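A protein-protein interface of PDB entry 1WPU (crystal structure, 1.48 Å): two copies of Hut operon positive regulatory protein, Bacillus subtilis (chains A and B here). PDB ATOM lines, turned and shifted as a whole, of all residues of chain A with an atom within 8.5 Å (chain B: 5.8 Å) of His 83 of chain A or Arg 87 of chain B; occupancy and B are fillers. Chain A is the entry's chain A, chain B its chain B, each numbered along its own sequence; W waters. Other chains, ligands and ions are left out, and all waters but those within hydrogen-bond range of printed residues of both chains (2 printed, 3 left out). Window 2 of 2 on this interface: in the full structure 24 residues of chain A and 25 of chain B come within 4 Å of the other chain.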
ATOM      1  N   HIS A  76     -10.907   6.942 -23.417  1.00  0.00           N
ATOM      2  CA  HIS A  76     -10.242   7.778 -22.431  1.00  0.00           C
ATOM      3  C   HIS A  76     -11.065   8.995 -22.039  1.00  0.00           C
ATOM      4  O   HIS A  76     -11.023   9.418 -20.888  1.00  0.00           O
ATOM      5  CB  HIS A  76      -8.856   8.146 -22.937  1.00  0.00           C
ATOM      6  CG  HIS A  76      -7.879   7.026 -22.793  1.00  0.00           C
ATOM      7  ND1 HIS A  76      -7.338   6.670 -21.575  1.00  0.00           N
ATOM      8  CD2 HIS A  76      -7.404   6.131 -23.691  1.00  0.00           C
ATOM      9  CE1 HIS A  76      -6.571   5.606 -21.733  1.00  0.00           C
ATOM     10  NE2 HIS A  76      -6.596   5.260 -23.007  1.00  0.00           N
ATOM     11  N   ALA A  77     -11.837   9.538 -22.977  1.00  0.00           N
ATOM     12  CA  ALA A  77     -12.701  10.672 -22.658  1.00  0.00           C
ATOM     13  C   ALA A  77     -13.785  10.186 -21.686  1.00  0.00           C
ATOM     14  O   ALA A  77     -14.173  10.894 -20.750  1.00  0.00           O
ATOM     15  CB  ALA A  77     -13.341  11.229 -23.930  1.00  0.00           C
ATOM     16  N   THR A  78     -14.277   8.969 -21.908  1.00  0.00           N
ATOM     17  CA  THR A  78     -15.298   8.413 -21.036  1.00  0.00           C
ATOM     18  C   THR A  78     -14.725   8.180 -19.637  1.00  0.00           C
ATOM     19  O   THR A  78     -15.392   8.445 -18.636  1.00  0.00           O
ATOM     20  CB  THR A  78     -15.844   7.096 -21.603  1.00  0.00           C
ATOM     21  OG1 THR A  78     -16.435   7.350 -22.885  1.00  0.00           O
ATOM     22  CG2 THR A  78     -16.899   6.519 -20.681  1.00  0.00           C
ATOM     23  N   MET A  79     -13.489   7.691 -19.575  1.00  0.00           N
ATOM     24  CA  MET A  79     -12.825   7.452 -18.293  1.00  0.00           C
ATOM     25  C   MET A  79     -12.712   8.759 -17.518  1.00  0.00           C
ATOM     26  O   MET A  79     -12.983   8.809 -16.318  1.00  0.00           O
ATOM     27  CB  MET A  79     -11.420   6.883 -18.507  1.00  0.00           C
ATOM     28  CG  MET A  79     -11.363   5.462 -19.034  1.00  0.00           C
ATOM     29  SD  MET A  79     -12.052   4.267 -17.882  1.00  0.00           S
ATOM     30  CE  MET A  79     -13.681   4.193 -18.469  1.00  0.00           C
ATOM     31  N   GLU A  80     -12.320   9.825 -18.208  1.00  0.00           N
ATOM     32  CA  GLU A  80     -12.177  11.108 -17.538  1.00  0.00           C
ATOM     33  C   GLU A  80     -13.520  11.608 -17.024  1.00  0.00           C
ATOM     34  O   GLU A  80     -13.599  12.167 -15.929  1.00  0.00           O
ATOM     35  CB  GLU A  80     -11.527  12.132 -18.473  1.00  0.00           C
ATOM     36  CG  GLU A  80     -10.102  11.758 -18.868  1.00  0.00           C
ATOM     37  CD  GLU A  80      -9.276  12.945 -19.324  1.00  0.00           C
ATOM     38  OE1 GLU A  80      -9.876  13.931 -19.786  1.00  0.00           O
ATOM     39  N   ALA A  81     -14.580  11.402 -17.804  1.00  0.00           N
ATOM     40  CA  ALA A  81     -15.911  11.822 -17.378  1.00  0.00           C
ATOM     41  C   ALA A  81     -16.338  11.015 -16.151  1.00  0.00           C
ATOM     42  O   ALA A  81     -16.975  11.544 -15.240  1.00  0.00           O
ATOM     43  CB  ALA A  81     -16.920  11.627 -18.515  1.00  0.00           C
ATOM     44  N   LEU A  82     -15.983   9.732 -16.123  1.00  0.00           N
ATOM     45  CA  LEU A  82     -16.351   8.886 -14.995  1.00  0.00           C
ATOM     46  C   LEU A  82     -15.674   9.307 -13.699  1.00  0.00           C
ATOM     47  O   LEU A  82     -16.179   9.016 -12.612  1.00  0.00           O
ATOM     48  CB  LEU A  82     -16.040   7.420 -15.306  1.00  0.00           C
ATOM     49  CG  LEU A  82     -17.057   6.797 -16.263  1.00  0.00           C
ATOM     50  CD1 LEU A  82     -16.632   5.376 -16.591  1.00  0.00           C
ATOM     51  CD2 LEU A  82     -18.445   6.816 -15.630  1.00  0.00           C
ATOM     52  N   HIS A  83     -14.537   9.990 -13.795  1.00  0.00           N
ATOM     53  CA  HIS A  83     -13.851  10.453 -12.587  1.00  0.00           C
ATOM     54  C   HIS A  83     -14.725  11.436 -11.817  1.00  0.00           C
ATOM     55  O   HIS A  83     -14.774  11.409 -10.584  1.00  0.00           O
ATOM     56  CB  HIS A  83     -12.528  11.137 -12.934  1.00  0.00           C
ATOM     57  CG  HIS A  83     -11.351  10.219 -12.893  1.00  0.00           C
ATOM     58  ND1 HIS A  83     -10.735   9.744 -14.031  1.00  0.00           N
ATOM     59  CD2 HIS A  83     -10.683   9.676 -11.849  1.00  0.00           C
ATOM     60  CE1 HIS A  83      -9.735   8.950 -13.689  1.00  0.00           C
ATOM     61  NE2 HIS A  83      -9.683   8.892 -12.370  1.00  0.00           N
ATOM     62  N   GLY A  84     -15.405  12.316 -12.545  1.00  0.00           N
ATOM     63  CA  GLY A  84     -16.267  13.288 -11.902  1.00  0.00           C
ATOM     64  C   GLY A  84     -17.470  12.625 -11.269  1.00  0.00           C
ATOM     65  O   GLY A  84     -17.979  13.068 -10.240  1.00  0.00           O
ATOM     66  N   VAL A  85     -17.928  11.544 -11.889  1.00  0.00           N
ATOM     67  CA  VAL A  85     -19.076  10.818 -11.385  1.00  0.00           C
ATOM     68  C   VAL A  85     -18.747   9.968 -10.164  1.00  0.00           C
ATOM     69  O   VAL A  85     -19.509   9.955  -9.198  1.00  0.00           O
ATOM     70  CB  VAL A  85     -19.677   9.904 -12.483  1.00  0.00           C
ATOM     71  CG1 VAL A  85     -20.735   8.975 -11.888  1.00  0.00           C
ATOM     72  CG2 VAL A  85     -20.281  10.761 -13.588  1.00  0.00           C
ATOM     73  N   THR A  86     -17.612   9.272 -10.202  1.00  0.00           N
ATOM     74  CA  THR A  86     -17.226   8.383  -9.106  1.00  0.00           C
ATOM     75  C   THR A  86     -16.377   9.011  -8.001  1.00  0.00           C
ATOM     76  O   THR A  86     -16.336   8.498  -6.885  1.00  0.00           O
ATOM     77  CB  THR A  86     -16.517   7.129  -9.647  1.00  0.00           C
ATOM     78  OG1 THR A  86     -15.375   7.516 -10.414  1.00  0.00           O
ATOM     79  CG2 THR A  86     -17.465   6.328 -10.537  1.00  0.00           C
ATOM     80  N   ARG A  87     -15.684  10.100  -8.319  1.00  0.00           N
ATOM     81  CA  ARG A  87     -14.882  10.835  -7.336  1.00  0.00           C
ATOM     82  C   ARG A  87     -13.941  10.055  -6.413  1.00  0.00           C
ATOM     83  O   ARG A  87     -14.065  10.137  -5.190  1.00  0.00           O
ATOM     84  CB  ARG A  87     -15.817  11.703  -6.485  1.00  0.00           C
ATOM     85  CG  ARG A  87     -16.458  12.856  -7.249  1.00  0.00           C
ATOM     86  CD  ARG A  87     -17.880  13.130  -6.764  1.00  0.00           C
ATOM     87  NE  ARG A  87     -18.725  11.965  -7.021  1.00  0.00           N
ATOM     88  CZ  ARG A  87     -19.418  11.317  -6.095  1.00  0.00           C
ATOM     89  NH1 ARG A  87     -19.393  11.715  -4.832  1.00  0.00           N
ATOM     90  NH2 ARG A  87     -20.099  10.230  -6.429  1.00  0.00           N
ATOM     91  N   GLY A  88     -12.998   9.316  -6.986  1.00  0.00           N
ATOM     92  CA  GLY A  88     -12.053   8.592  -6.153  1.00  0.00           C
ATOM     93  C   GLY A  88     -11.851   7.137  -6.507  1.00  0.00           C
ATOM     94  O   GLY A  88     -10.726   6.687  -6.724  1.00  0.00           O
ATOM     95  N   GLU A  89     -12.944   6.389  -6.541  1.00  0.00           N
ATOM     96  CA  GLU A  89     -12.893   4.974  -6.877  1.00  0.00           C
ATOM     97  C   GLU A  89     -13.852   4.764  -8.035  1.00  0.00           C
ATOM     98  O   GLU A  89     -15.049   5.017  -7.901  1.00  0.00           O
ATOM     99  CB  GLU A  89     -13.332   4.120  -5.686  1.00  0.00           C
ATOM    100  CG  GLU A  89     -12.417   4.205  -4.473  1.00  0.00           C
ATOM    101  CD  GLU A  89     -11.009   3.727  -4.769  1.00  0.00           C
ATOM    102  OE1 GLU A  89     -10.845   2.570  -5.218  1.00  0.00           O
ATOM    103  OE2 GLU A  89     -10.062   4.510  -4.546  1.00  0.00           O
ATOM    104  N   MET A  90     -13.334   4.308  -9.170  1.00  0.00           N
ATOM    105  CA  MET A  90     -14.178   4.103 -10.340  1.00  0.00           C
ATOM    106  C   MET A  90     -14.921   2.782 -10.197  1.00  0.00           C
ATOM    107  O   MET A  90     -14.744   1.861 -10.993  1.00  0.00           O
ATOM    108  CB  MET A  90     -13.333   4.110 -11.616  1.00  0.00           C
ATOM    109  CG  MET A  90     -14.090   4.628 -12.829  1.00  0.00           C
ATOM    110  SD  MET A  90     -13.020   4.997 -14.227  1.00  0.00           S
ATOM    111  CE  MET A  90     -12.360   6.597 -13.725  1.00  0.00           C
ATOM    112  N   ARG A  97     -23.185   1.057  -4.683  1.00  0.00           N
ATOM    113  CA  ARG A  97     -23.845   2.232  -5.225  1.00  0.00           C
ATOM    114  C   ARG A  97     -24.226   2.004  -6.677  1.00  0.00           C
ATOM    115  O   ARG A  97     -23.659   1.150  -7.368  1.00  0.00           O
ATOM    116  CB  ARG A  97     -22.994   3.500  -5.060  1.00  0.00           C
ATOM    117  CG  ARG A  97     -21.675   3.514  -5.778  1.00  0.00           C
ATOM    118  CD  ARG A  97     -20.903   4.792  -5.443  1.00  0.00           C
ATOM    119  NE  ARG A  97     -19.589   4.770  -6.071  1.00  0.00           N
ATOM    120  CZ  ARG A  97     -18.699   5.754  -5.998  1.00  0.00           C
ATOM    121  NH1 ARG A  97     -18.970   6.866  -5.328  1.00  0.00           N
ATOM    122  NH2 ARG A  97     -17.518   5.607  -6.582  1.00  0.00           N
ATOM    123  N   LEU A 124     -21.706  13.609 -18.586  1.00  0.00           N
ATOM    124  CA  LEU A 124     -22.624  12.764 -17.844  1.00  0.00           C
ATOM    125  C   LEU A 124     -23.331  13.535 -16.747  1.00  0.00           C
ATOM    126  O   LEU A 124     -22.723  14.360 -16.063  1.00  0.00           O
ATOM    127  CB  LEU A 124     -21.848  11.614 -17.196  1.00  0.00           C
ATOM    128  CG  LEU A 124     -20.864  10.851 -18.084  1.00  0.00           C
ATOM    129  CD1 LEU A 124     -20.045   9.873 -17.252  1.00  0.00           C
ATOM    130  CD2 LEU A 124     -21.630  10.124 -19.172  1.00  0.00           C
ATOM    131  N   THR A 139     -24.916  13.764  -9.705  1.00  0.00           N
ATOM    132  CA  THR A 139     -23.537  13.487 -10.068  1.00  0.00           C
ATOM    133  C   THR A 139     -23.313  14.014 -11.483  1.00  0.00           C
ATOM    134  O   THR A 139     -24.241  14.025 -12.303  1.00  0.00           O
ATOM    135  CB  THR A 139     -23.232  11.972  -9.976  1.00  0.00           C
ATOM    136  OG1 THR A 139     -21.824  11.759 -10.137  1.00  0.00           O
ATOM    137  CG2 THR A 139     -24.007  11.188 -11.036  1.00  0.00           C
ATOM    138  N   PHE A 140     -22.092  14.477 -11.747  1.00  0.00           N
ATOM    139  CA  PHE A 140     -21.707  15.044 -13.039  1.00  0.00           C
ATOM    140  C   PHE A 140     -20.303  14.605 -13.412  1.00  0.00           C
ATOM    141  O   PHE A 140     -19.473  14.338 -12.542  1.00  0.00           O
ATOM    142  CB  PHE A 140     -21.633  16.574 -12.998  1.00  0.00           C
ATOM    143  CG  PHE A 140     -22.942  17.277 -12.840  1.00  0.00           C
ATOM    144  CD1 PHE A 140     -23.599  17.303 -11.614  1.00  0.00           C
ATOM    145  CD2 PHE A 140     -23.463  18.020 -13.897  1.00  0.00           C
ATOM    146  CE1 PHE A 140     -24.752  18.071 -11.442  1.00  0.00           C
ATOM    147  CE2 PHE A 140     -24.609  18.787 -13.734  1.00  0.00           C
ATOM    148  CZ  PHE A 140     -25.253  18.814 -12.505  1.00  0.00           C
ATOM    149  N   GLY A 141     -20.026  14.590 -14.711  1.00  0.00           N
ATOM    150  CA  GLY A 141     -18.699  14.236 -15.177  1.00  0.00           C
ATOM    151  C   GLY A 141     -18.493  14.691 -16.610  1.00  0.00           C
ATOM    152  O   GLY A 141     -19.378  14.523 -17.441  1.00  0.00           O
ATOM    153  N   VAL A 142     -17.340  15.288 -16.898  1.00  0.00           N
ATOM    154  CA  VAL A 142     -17.023  15.723 -18.254  1.00  0.00           C
ATOM    155  C   VAL A 142     -15.591  15.323 -18.590  1.00  0.00           C
ATOM    156  O   VAL A 142     -14.664  15.585 -17.814  1.00  0.00           O
ATOM    157  CB  VAL A 142     -17.158  17.257 -18.424  1.00  0.00           C
ATOM    158  CG1 VAL A 142     -16.815  17.654 -19.868  1.00  0.00           C
ATOM    159  CG2 VAL A 142     -18.575  17.696 -18.079  1.00  0.00           C
ATOM    160  N   GLY A 143     -15.428  14.659 -19.732  1.00  0.00           N
ATOM    161  CA  GLY A 143     -14.114  14.251 -20.191  1.00  0.00           C
ATOM    162  C   GLY A 143     -13.898  14.819 -21.582  1.00  0.00           C
ATOM    163  O   GLY A 143     -14.814  14.802 -22.404  1.00  0.00           O
ATOM    164  N   ILE A 144     -12.696  15.323 -21.846  1.00  0.00           N
ATOM    165  CA  ILE A 144     -12.362  15.913 -23.141  1.00  0.00           C
ATOM    166  C   ILE A 144     -11.071  15.297 -23.674  1.00  0.00           C
ATOM    167  O   ILE A 144     -10.116  15.104 -22.925  1.00  0.00           O
ATOM    168  CB  ILE A 144     -12.204  17.454 -23.007  1.00  0.00           C
ATOM    169  CG1 ILE A 144     -13.563  18.079 -22.671  1.00  0.00           C
ATOM    170  CG2 ILE A 144     -11.652  18.047 -24.299  1.00  0.00           C
ATOM    171  CD1 ILE A 144     -13.531  19.575 -22.453  1.00  0.00           C
ATOM    172  N   ASN A 145     -11.041  14.986 -24.966  1.00  0.00           N
ATOM    173  CA  ASN A 145      -9.859  14.372 -25.568  1.00  0.00           C
ATOM    174  C   ASN A 145      -9.746  14.756 -27.036  1.00  0.00           C
ATOM    175  O   ASN A 145     -10.730  15.170 -27.646  1.00  0.00           O
ATOM    176  CB  ASN A 145      -9.960  12.842 -25.446  1.00  0.00           C
ATOM    177  CG  ASN A 145      -8.610  12.156 -25.492  1.00  0.00           C
ATOM    178  OD1 ASN A 145      -7.562  12.807 -25.449  1.00  0.00           O
ATOM    179  ND2 ASN A 145      -8.625  10.826 -25.561  1.00  0.00           N
ATOM    180  N   LEU B  82     -13.243  18.860  -7.131  1.00  0.00           N
ATOM    181  CA  LEU B  82     -11.899  18.869  -7.692  1.00  0.00           C
ATOM    182  C   LEU B  82     -11.558  17.573  -8.410  1.00  0.00           C
ATOM    183  O   LEU B  82     -10.695  17.564  -9.289  1.00  0.00           O
ATOM    184  CB  LEU B  82     -10.861  19.160  -6.605  1.00  0.00           C
ATOM    185  CG  LEU B  82     -10.812  20.642  -6.229  1.00  0.00           C
ATOM    186  CD1 LEU B  82      -9.858  20.835  -5.059  1.00  0.00           C
ATOM    187  CD2 LEU B  82     -10.369  21.471  -7.431  1.00  0.00           C
ATOM    188  N   HIS B  83     -12.227  16.481  -8.051  1.00  0.00           N
ATOM    189  CA  HIS B  83     -11.964  15.210  -8.723  1.00  0.00           C
ATOM    190  C   HIS B  83     -12.332  15.299 -10.194  1.00  0.00           C
ATOM    191  O   HIS B  83     -11.635  14.749 -11.051  1.00  0.00           O
ATOM    192  CB  HIS B  83     -12.763  14.073  -8.086  1.00  0.00           C
ATOM    193  CG  HIS B  83     -12.025  13.350  -7.007  1.00  0.00           C
ATOM    194  ND1 HIS B  83     -12.293  13.533  -5.668  1.00  0.00           N
ATOM    195  CD2 HIS B  83     -11.022  12.443  -7.071  1.00  0.00           C
ATOM    196  CE1 HIS B  83     -11.487  12.767  -4.952  1.00  0.00           C
ATOM    197  NE2 HIS B  83     -10.706  12.097  -5.780  1.00  0.00           N
ATOM    198  N   GLY B  84     -13.428  15.991 -10.489  1.00  0.00           N
ATOM    199  CA  GLY B  84     -13.861  16.130 -11.867  1.00  0.00           C
ATOM    200  C   GLY B  84     -12.902  17.003 -12.643  1.00  0.00           C
ATOM    201  O   GLY B  84     -12.680  16.809 -13.838  1.00  0.00           O
ATOM    202  N   VAL B  85     -12.317  17.971 -11.950  1.00  0.00           N
ATOM    203  CA  VAL B  85     -11.380  18.884 -12.579  1.00  0.00           C
ATOM    204  C   VAL B  85     -10.010  18.261 -12.828  1.00  0.00           C
ATOM    205  O   VAL B  85      -9.438  18.436 -13.902  1.00  0.00           O
ATOM    206  CB  VAL B  85     -11.203  20.164 -11.723  1.00  0.00           C
ATOM    207  CG1 VAL B  85     -10.056  21.019 -12.259  1.00  0.00           C
ATOM    208  CG2 VAL B  85     -12.503  20.965 -11.721  1.00  0.00           C
ATOM    209  N   THR B  86      -9.501  17.522 -11.845  1.00  0.00           N
ATOM    210  CA  THR B  86      -8.173  16.922 -11.946  1.00  0.00           C
ATOM    211  C   THR B  86      -8.120  15.512 -12.531  1.00  0.00           C
ATOM    212  O   THR B  86      -7.080  15.088 -13.031  1.00  0.00           O
ATOM    213  CB  THR B  86      -7.468  16.938 -10.579  1.00  0.00           C
ATOM    214  OG1 THR B  86      -8.273  16.256  -9.617  1.00  0.00           O
ATOM    215  CG2 THR B  86      -7.239  18.379 -10.115  1.00  0.00           C
ATOM    216  N   ARG B  87      -9.230  14.784 -12.451  1.00  0.00           N
ATOM    217  CA  ARG B  87      -9.335  13.442 -13.027  1.00  0.00           C
ATOM    218  C   ARG B  87      -8.224  12.423 -12.758  1.00  0.00           C
ATOM    219  O   ARG B  87      -7.602  11.919 -13.693  1.00  0.00           O
ATOM    220  CB  ARG B  87      -9.546  13.571 -14.538  1.00  0.00           C
ATOM    221  CG  ARG B  87     -10.906  14.142 -14.923  1.00  0.00           C
ATOM    222  CD  ARG B  87     -10.817  15.010 -16.174  1.00  0.00           C
ATOM    223  NE  ARG B  87      -9.961  16.164 -15.909  1.00  0.00           N
ATOM    224  CZ  ARG B  87      -8.877  16.476 -16.607  1.00  0.00           C
ATOM    225  NH1 ARG B  87      -8.501  15.734 -17.638  1.00  0.00           N
ATOM    226  NH2 ARG B  87      -8.134  17.509 -16.237  1.00  0.00           N
ATOM    227  N   GLY B  88      -7.984  12.109 -11.491  1.00  0.00           N
ATOM    228  CA  GLY B  88      -6.975  11.111 -11.185  1.00  0.00           C
ATOM    229  C   GLY B  88      -5.947  11.526 -10.159  1.00  0.00           C
ATOM    230  O   GLY B  88      -5.723  10.820  -9.179  1.00  0.00           O
ATOM    231  N   GLU B  89      -5.307  12.664 -10.393  1.00  0.00           N
ATOM    232  CA  GLU B  89      -4.291  13.169  -9.481  1.00  0.00           C
ATOM    233  C   GLU B  89      -4.711  14.578  -9.097  1.00  0.00           C
ATOM    234  O   GLU B  89      -4.788  15.452  -9.961  1.00  0.00           O
ATOM    235  CB  GLU B  89      -2.925  13.228 -10.174  1.00  0.00           C
ATOM    236  CG  GLU B  89      -2.672  12.155 -11.233  1.00  0.00           C
ATOM    237  CD  GLU B  89      -2.919  10.750 -10.729  1.00  0.00           C
ATOM    238  OE1 GLU B  89      -2.453  10.427  -9.617  1.00  0.00           O
ATOM    239  OE2 GLU B  89      -3.567   9.966 -11.452  1.00  0.00           O
ATOM    240  N   ARG B  97       0.593  21.775 -14.751  1.00  0.00           N
ATOM    241  CA  ARG B  97      -0.658  22.263 -15.311  1.00  0.00           C
ATOM    242  C   ARG B  97      -1.258  23.346 -14.428  1.00  0.00           C
ATOM    243  O   ARG B  97      -0.953  23.450 -13.234  1.00  0.00           O
ATOM    244  CB  ARG B  97      -1.661  21.126 -15.563  1.00  0.00           C
ATOM    245  CG  ARG B  97      -2.108  20.351 -14.353  1.00  0.00           C
ATOM    246  CD  ARG B  97      -3.017  19.192 -14.765  1.00  0.00           C
ATOM    247  NE  ARG B  97      -3.408  18.412 -13.599  1.00  0.00           N
ATOM    248  CZ  ARG B  97      -4.212  17.354 -13.632  1.00  0.00           C
ATOM    249  NH1 ARG B  97      -4.730  16.938 -14.781  1.00  0.00           N
ATOM    250  NH2 ARG B  97      -4.474  16.698 -12.510  1.00  0.00           N
ATOM    251  N   ILE B 128      -8.139  23.926 -18.115  1.00  0.00           N
ATOM    252  CA  ILE B 128      -6.963  23.351 -17.482  1.00  0.00           C
ATOM    253  C   ILE B 128      -5.972  23.100 -18.617  1.00  0.00           C
ATOM    254  O   ILE B 128      -6.371  22.747 -19.725  1.00  0.00           O
ATOM    255  CB  ILE B 128      -7.314  22.027 -16.734  1.00  0.00           C
ATOM    256  CG1 ILE B 128      -6.111  21.542 -15.923  1.00  0.00           C
ATOM    257  CG2 ILE B 128      -7.769  20.955 -17.721  1.00  0.00           C
ATOM    258  CD1 ILE B 128      -6.481  20.458 -14.900  1.00  0.00           C
ATOM    259  N   HIS B 137      -7.766  22.964 -22.382  1.00  0.00           N
ATOM    260  CA  HIS B 137      -9.107  22.544 -22.762  1.00  0.00           C
ATOM    261  C   HIS B 137     -10.002  22.745 -21.546  1.00  0.00           C
ATOM    262  O   HIS B 137      -9.522  23.076 -20.457  1.00  0.00           O
ATOM    263  CB  HIS B 137      -9.166  21.098 -23.314  1.00  0.00           C
ATOM    264  CG  HIS B 137      -8.703  20.032 -22.371  1.00  0.00           C
ATOM    265  ND1 HIS B 137      -9.352  19.742 -21.187  1.00  0.00           N
ATOM    266  CD2 HIS B 137      -7.694  19.137 -22.476  1.00  0.00           C
ATOM    267  CE1 HIS B 137      -8.760  18.712 -20.607  1.00  0.00           C
ATOM    268  NE2 HIS B 137      -7.754  18.328 -21.367  1.00  0.00           N
ATOM    269  N   THR B 139     -12.664  22.109 -18.374  1.00  0.00           N
ATOM    270  CA  THR B 139     -12.691  21.217 -17.226  1.00  0.00           C
ATOM    271  C   THR B 139     -13.923  21.565 -16.389  1.00  0.00           C
ATOM    272  O   THR B 139     -14.353  22.726 -16.351  1.00  0.00           O
ATOM    273  CB  THR B 139     -11.391  21.340 -16.392  1.00  0.00           C
ATOM    274  OG1 THR B 139     -11.361  20.303 -15.405  1.00  0.00           O
ATOM    275  CG2 THR B 139     -11.297  22.702 -15.712  1.00  0.00           C
HETATM  276  O   HOH W   1     -16.360  15.770  -9.463  1.00  0.00           O
HETATM  277  O   HOH W   2     -13.392  17.792 -16.426  1.00  0.00           O
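The guanidinium group (NH1) of Arg 87 of chain B is in salt-bridge range of the side-chain carboxylate (OE1) of Glu 80 of chain A, 3.1 Å away.
The backbone carbonyl oxygen (O) of Met 79 of chain A lies within hydrogen-bond range of a ring nitrogen (ND1) of His 83 of chain A, at 3.3 Å. The backbone carbonyl oxygen (O) of Gly 84 of chain A lies close to the guanidinium group (NE) of Arg 87 of chain A (3.5 Å). The backbone carbonyl oxygen (O) of Val 85 of chain A sits at hydrogen-bond distance from the guanidinium group (NH2) of Arg 87 of chain A (2.8 Å). O of Gly 84 of chain B sits close to NE of Arg 87 of chain B (3.5 Å). The backbone carbonyl oxygen (O) of Val 85 of chain B is in hydrogen-bond range of the guanidinium group (NH2) of Arg 87 of chain B (2.8 Å).
Among the printed residues, pairs that only touch across the chains: His 83 of chain A with Arg 87 of chain B, His 83 of chain A with Gly 88 of chain B, Gly 84 of chain A with Gly 84 of chain B, Arg 87 of chain A with His 83 of chain B and Gly 88 of chain A with His 83 of chain B.
His 83 of chain A touches just these residues of chain B: Arg 87 (3.7 Å) and Gly 88 (3.7 Å). Printed residues of chain A within 4 Å of Arg 87 of chain B: Glu 80 (3.1 Å) and His 83 (3.7 Å). Printed residues of chain A within 4 Å of Gly 84 of chain B: Gly 84. Of the printed residues of chain A, His 83 of chain B touches Arg 87 (3.7 Å) and Gly 88 (3.7 Å). Of the printed residues of chain B, Arg 87 of chain A touches His 83 (3.7 Å). Of the printed residues of chain B, Glu 80 of chain A touches Arg 87 (3.1 Å). Ala 81 of chain A touches none of the printed residues of chain B. Thr 139 of chain B touches none of the printed residues of chain A. The nearest residue of chain B that does not touch His 83 of chain A is His 83 of chain B (4.2 Å). The nearest residue of chain A that does not touch Arg 87 of chain B is Val 142 of chain A (4.2 Å). The nearest printed residue of chain A that does not touch Gly 84 of chain B is Val 142 of chain A (4.6 Å).
Hydrophobic or aromatic side chains of chain A within 4 Å of the printed part of chain B: His 83. Among the printed residues, 6 pairs touch across the chains. Among the printed residues, Asp or Glu carboxylates within 4 Å of a Lys or Arg side-chain nitrogen of the other chain: Glu 80 of chain A with Arg 87 of chain B.
His 83 of chain A touches Arg 87 of chain B, and with the chains exchanged Arg 87 of chain A touches His 83 of chain B. His 83 of chain A touches Gly 88 of chain B, and with the chains exchanged Gly 88 of chain A touches His 83 of chain B. Gly 84 of chain B touches its own counterpart, Gly 84 of chain A. 10 positions are printed for both chains.
Water W2 lies within hydrogen-bond range of O of Gly 84 of chain B (2.9 Å), O of Val 142 of chain A (2.9 Å) and OG1 of Thr 139 of chain B (3.4 Å). Water W1 bridges the backbone NH of Gly 84 of chain B (3.1 Å) and the backbone carbonyl oxygen of Gly 84 of chain A (3.2 Å).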
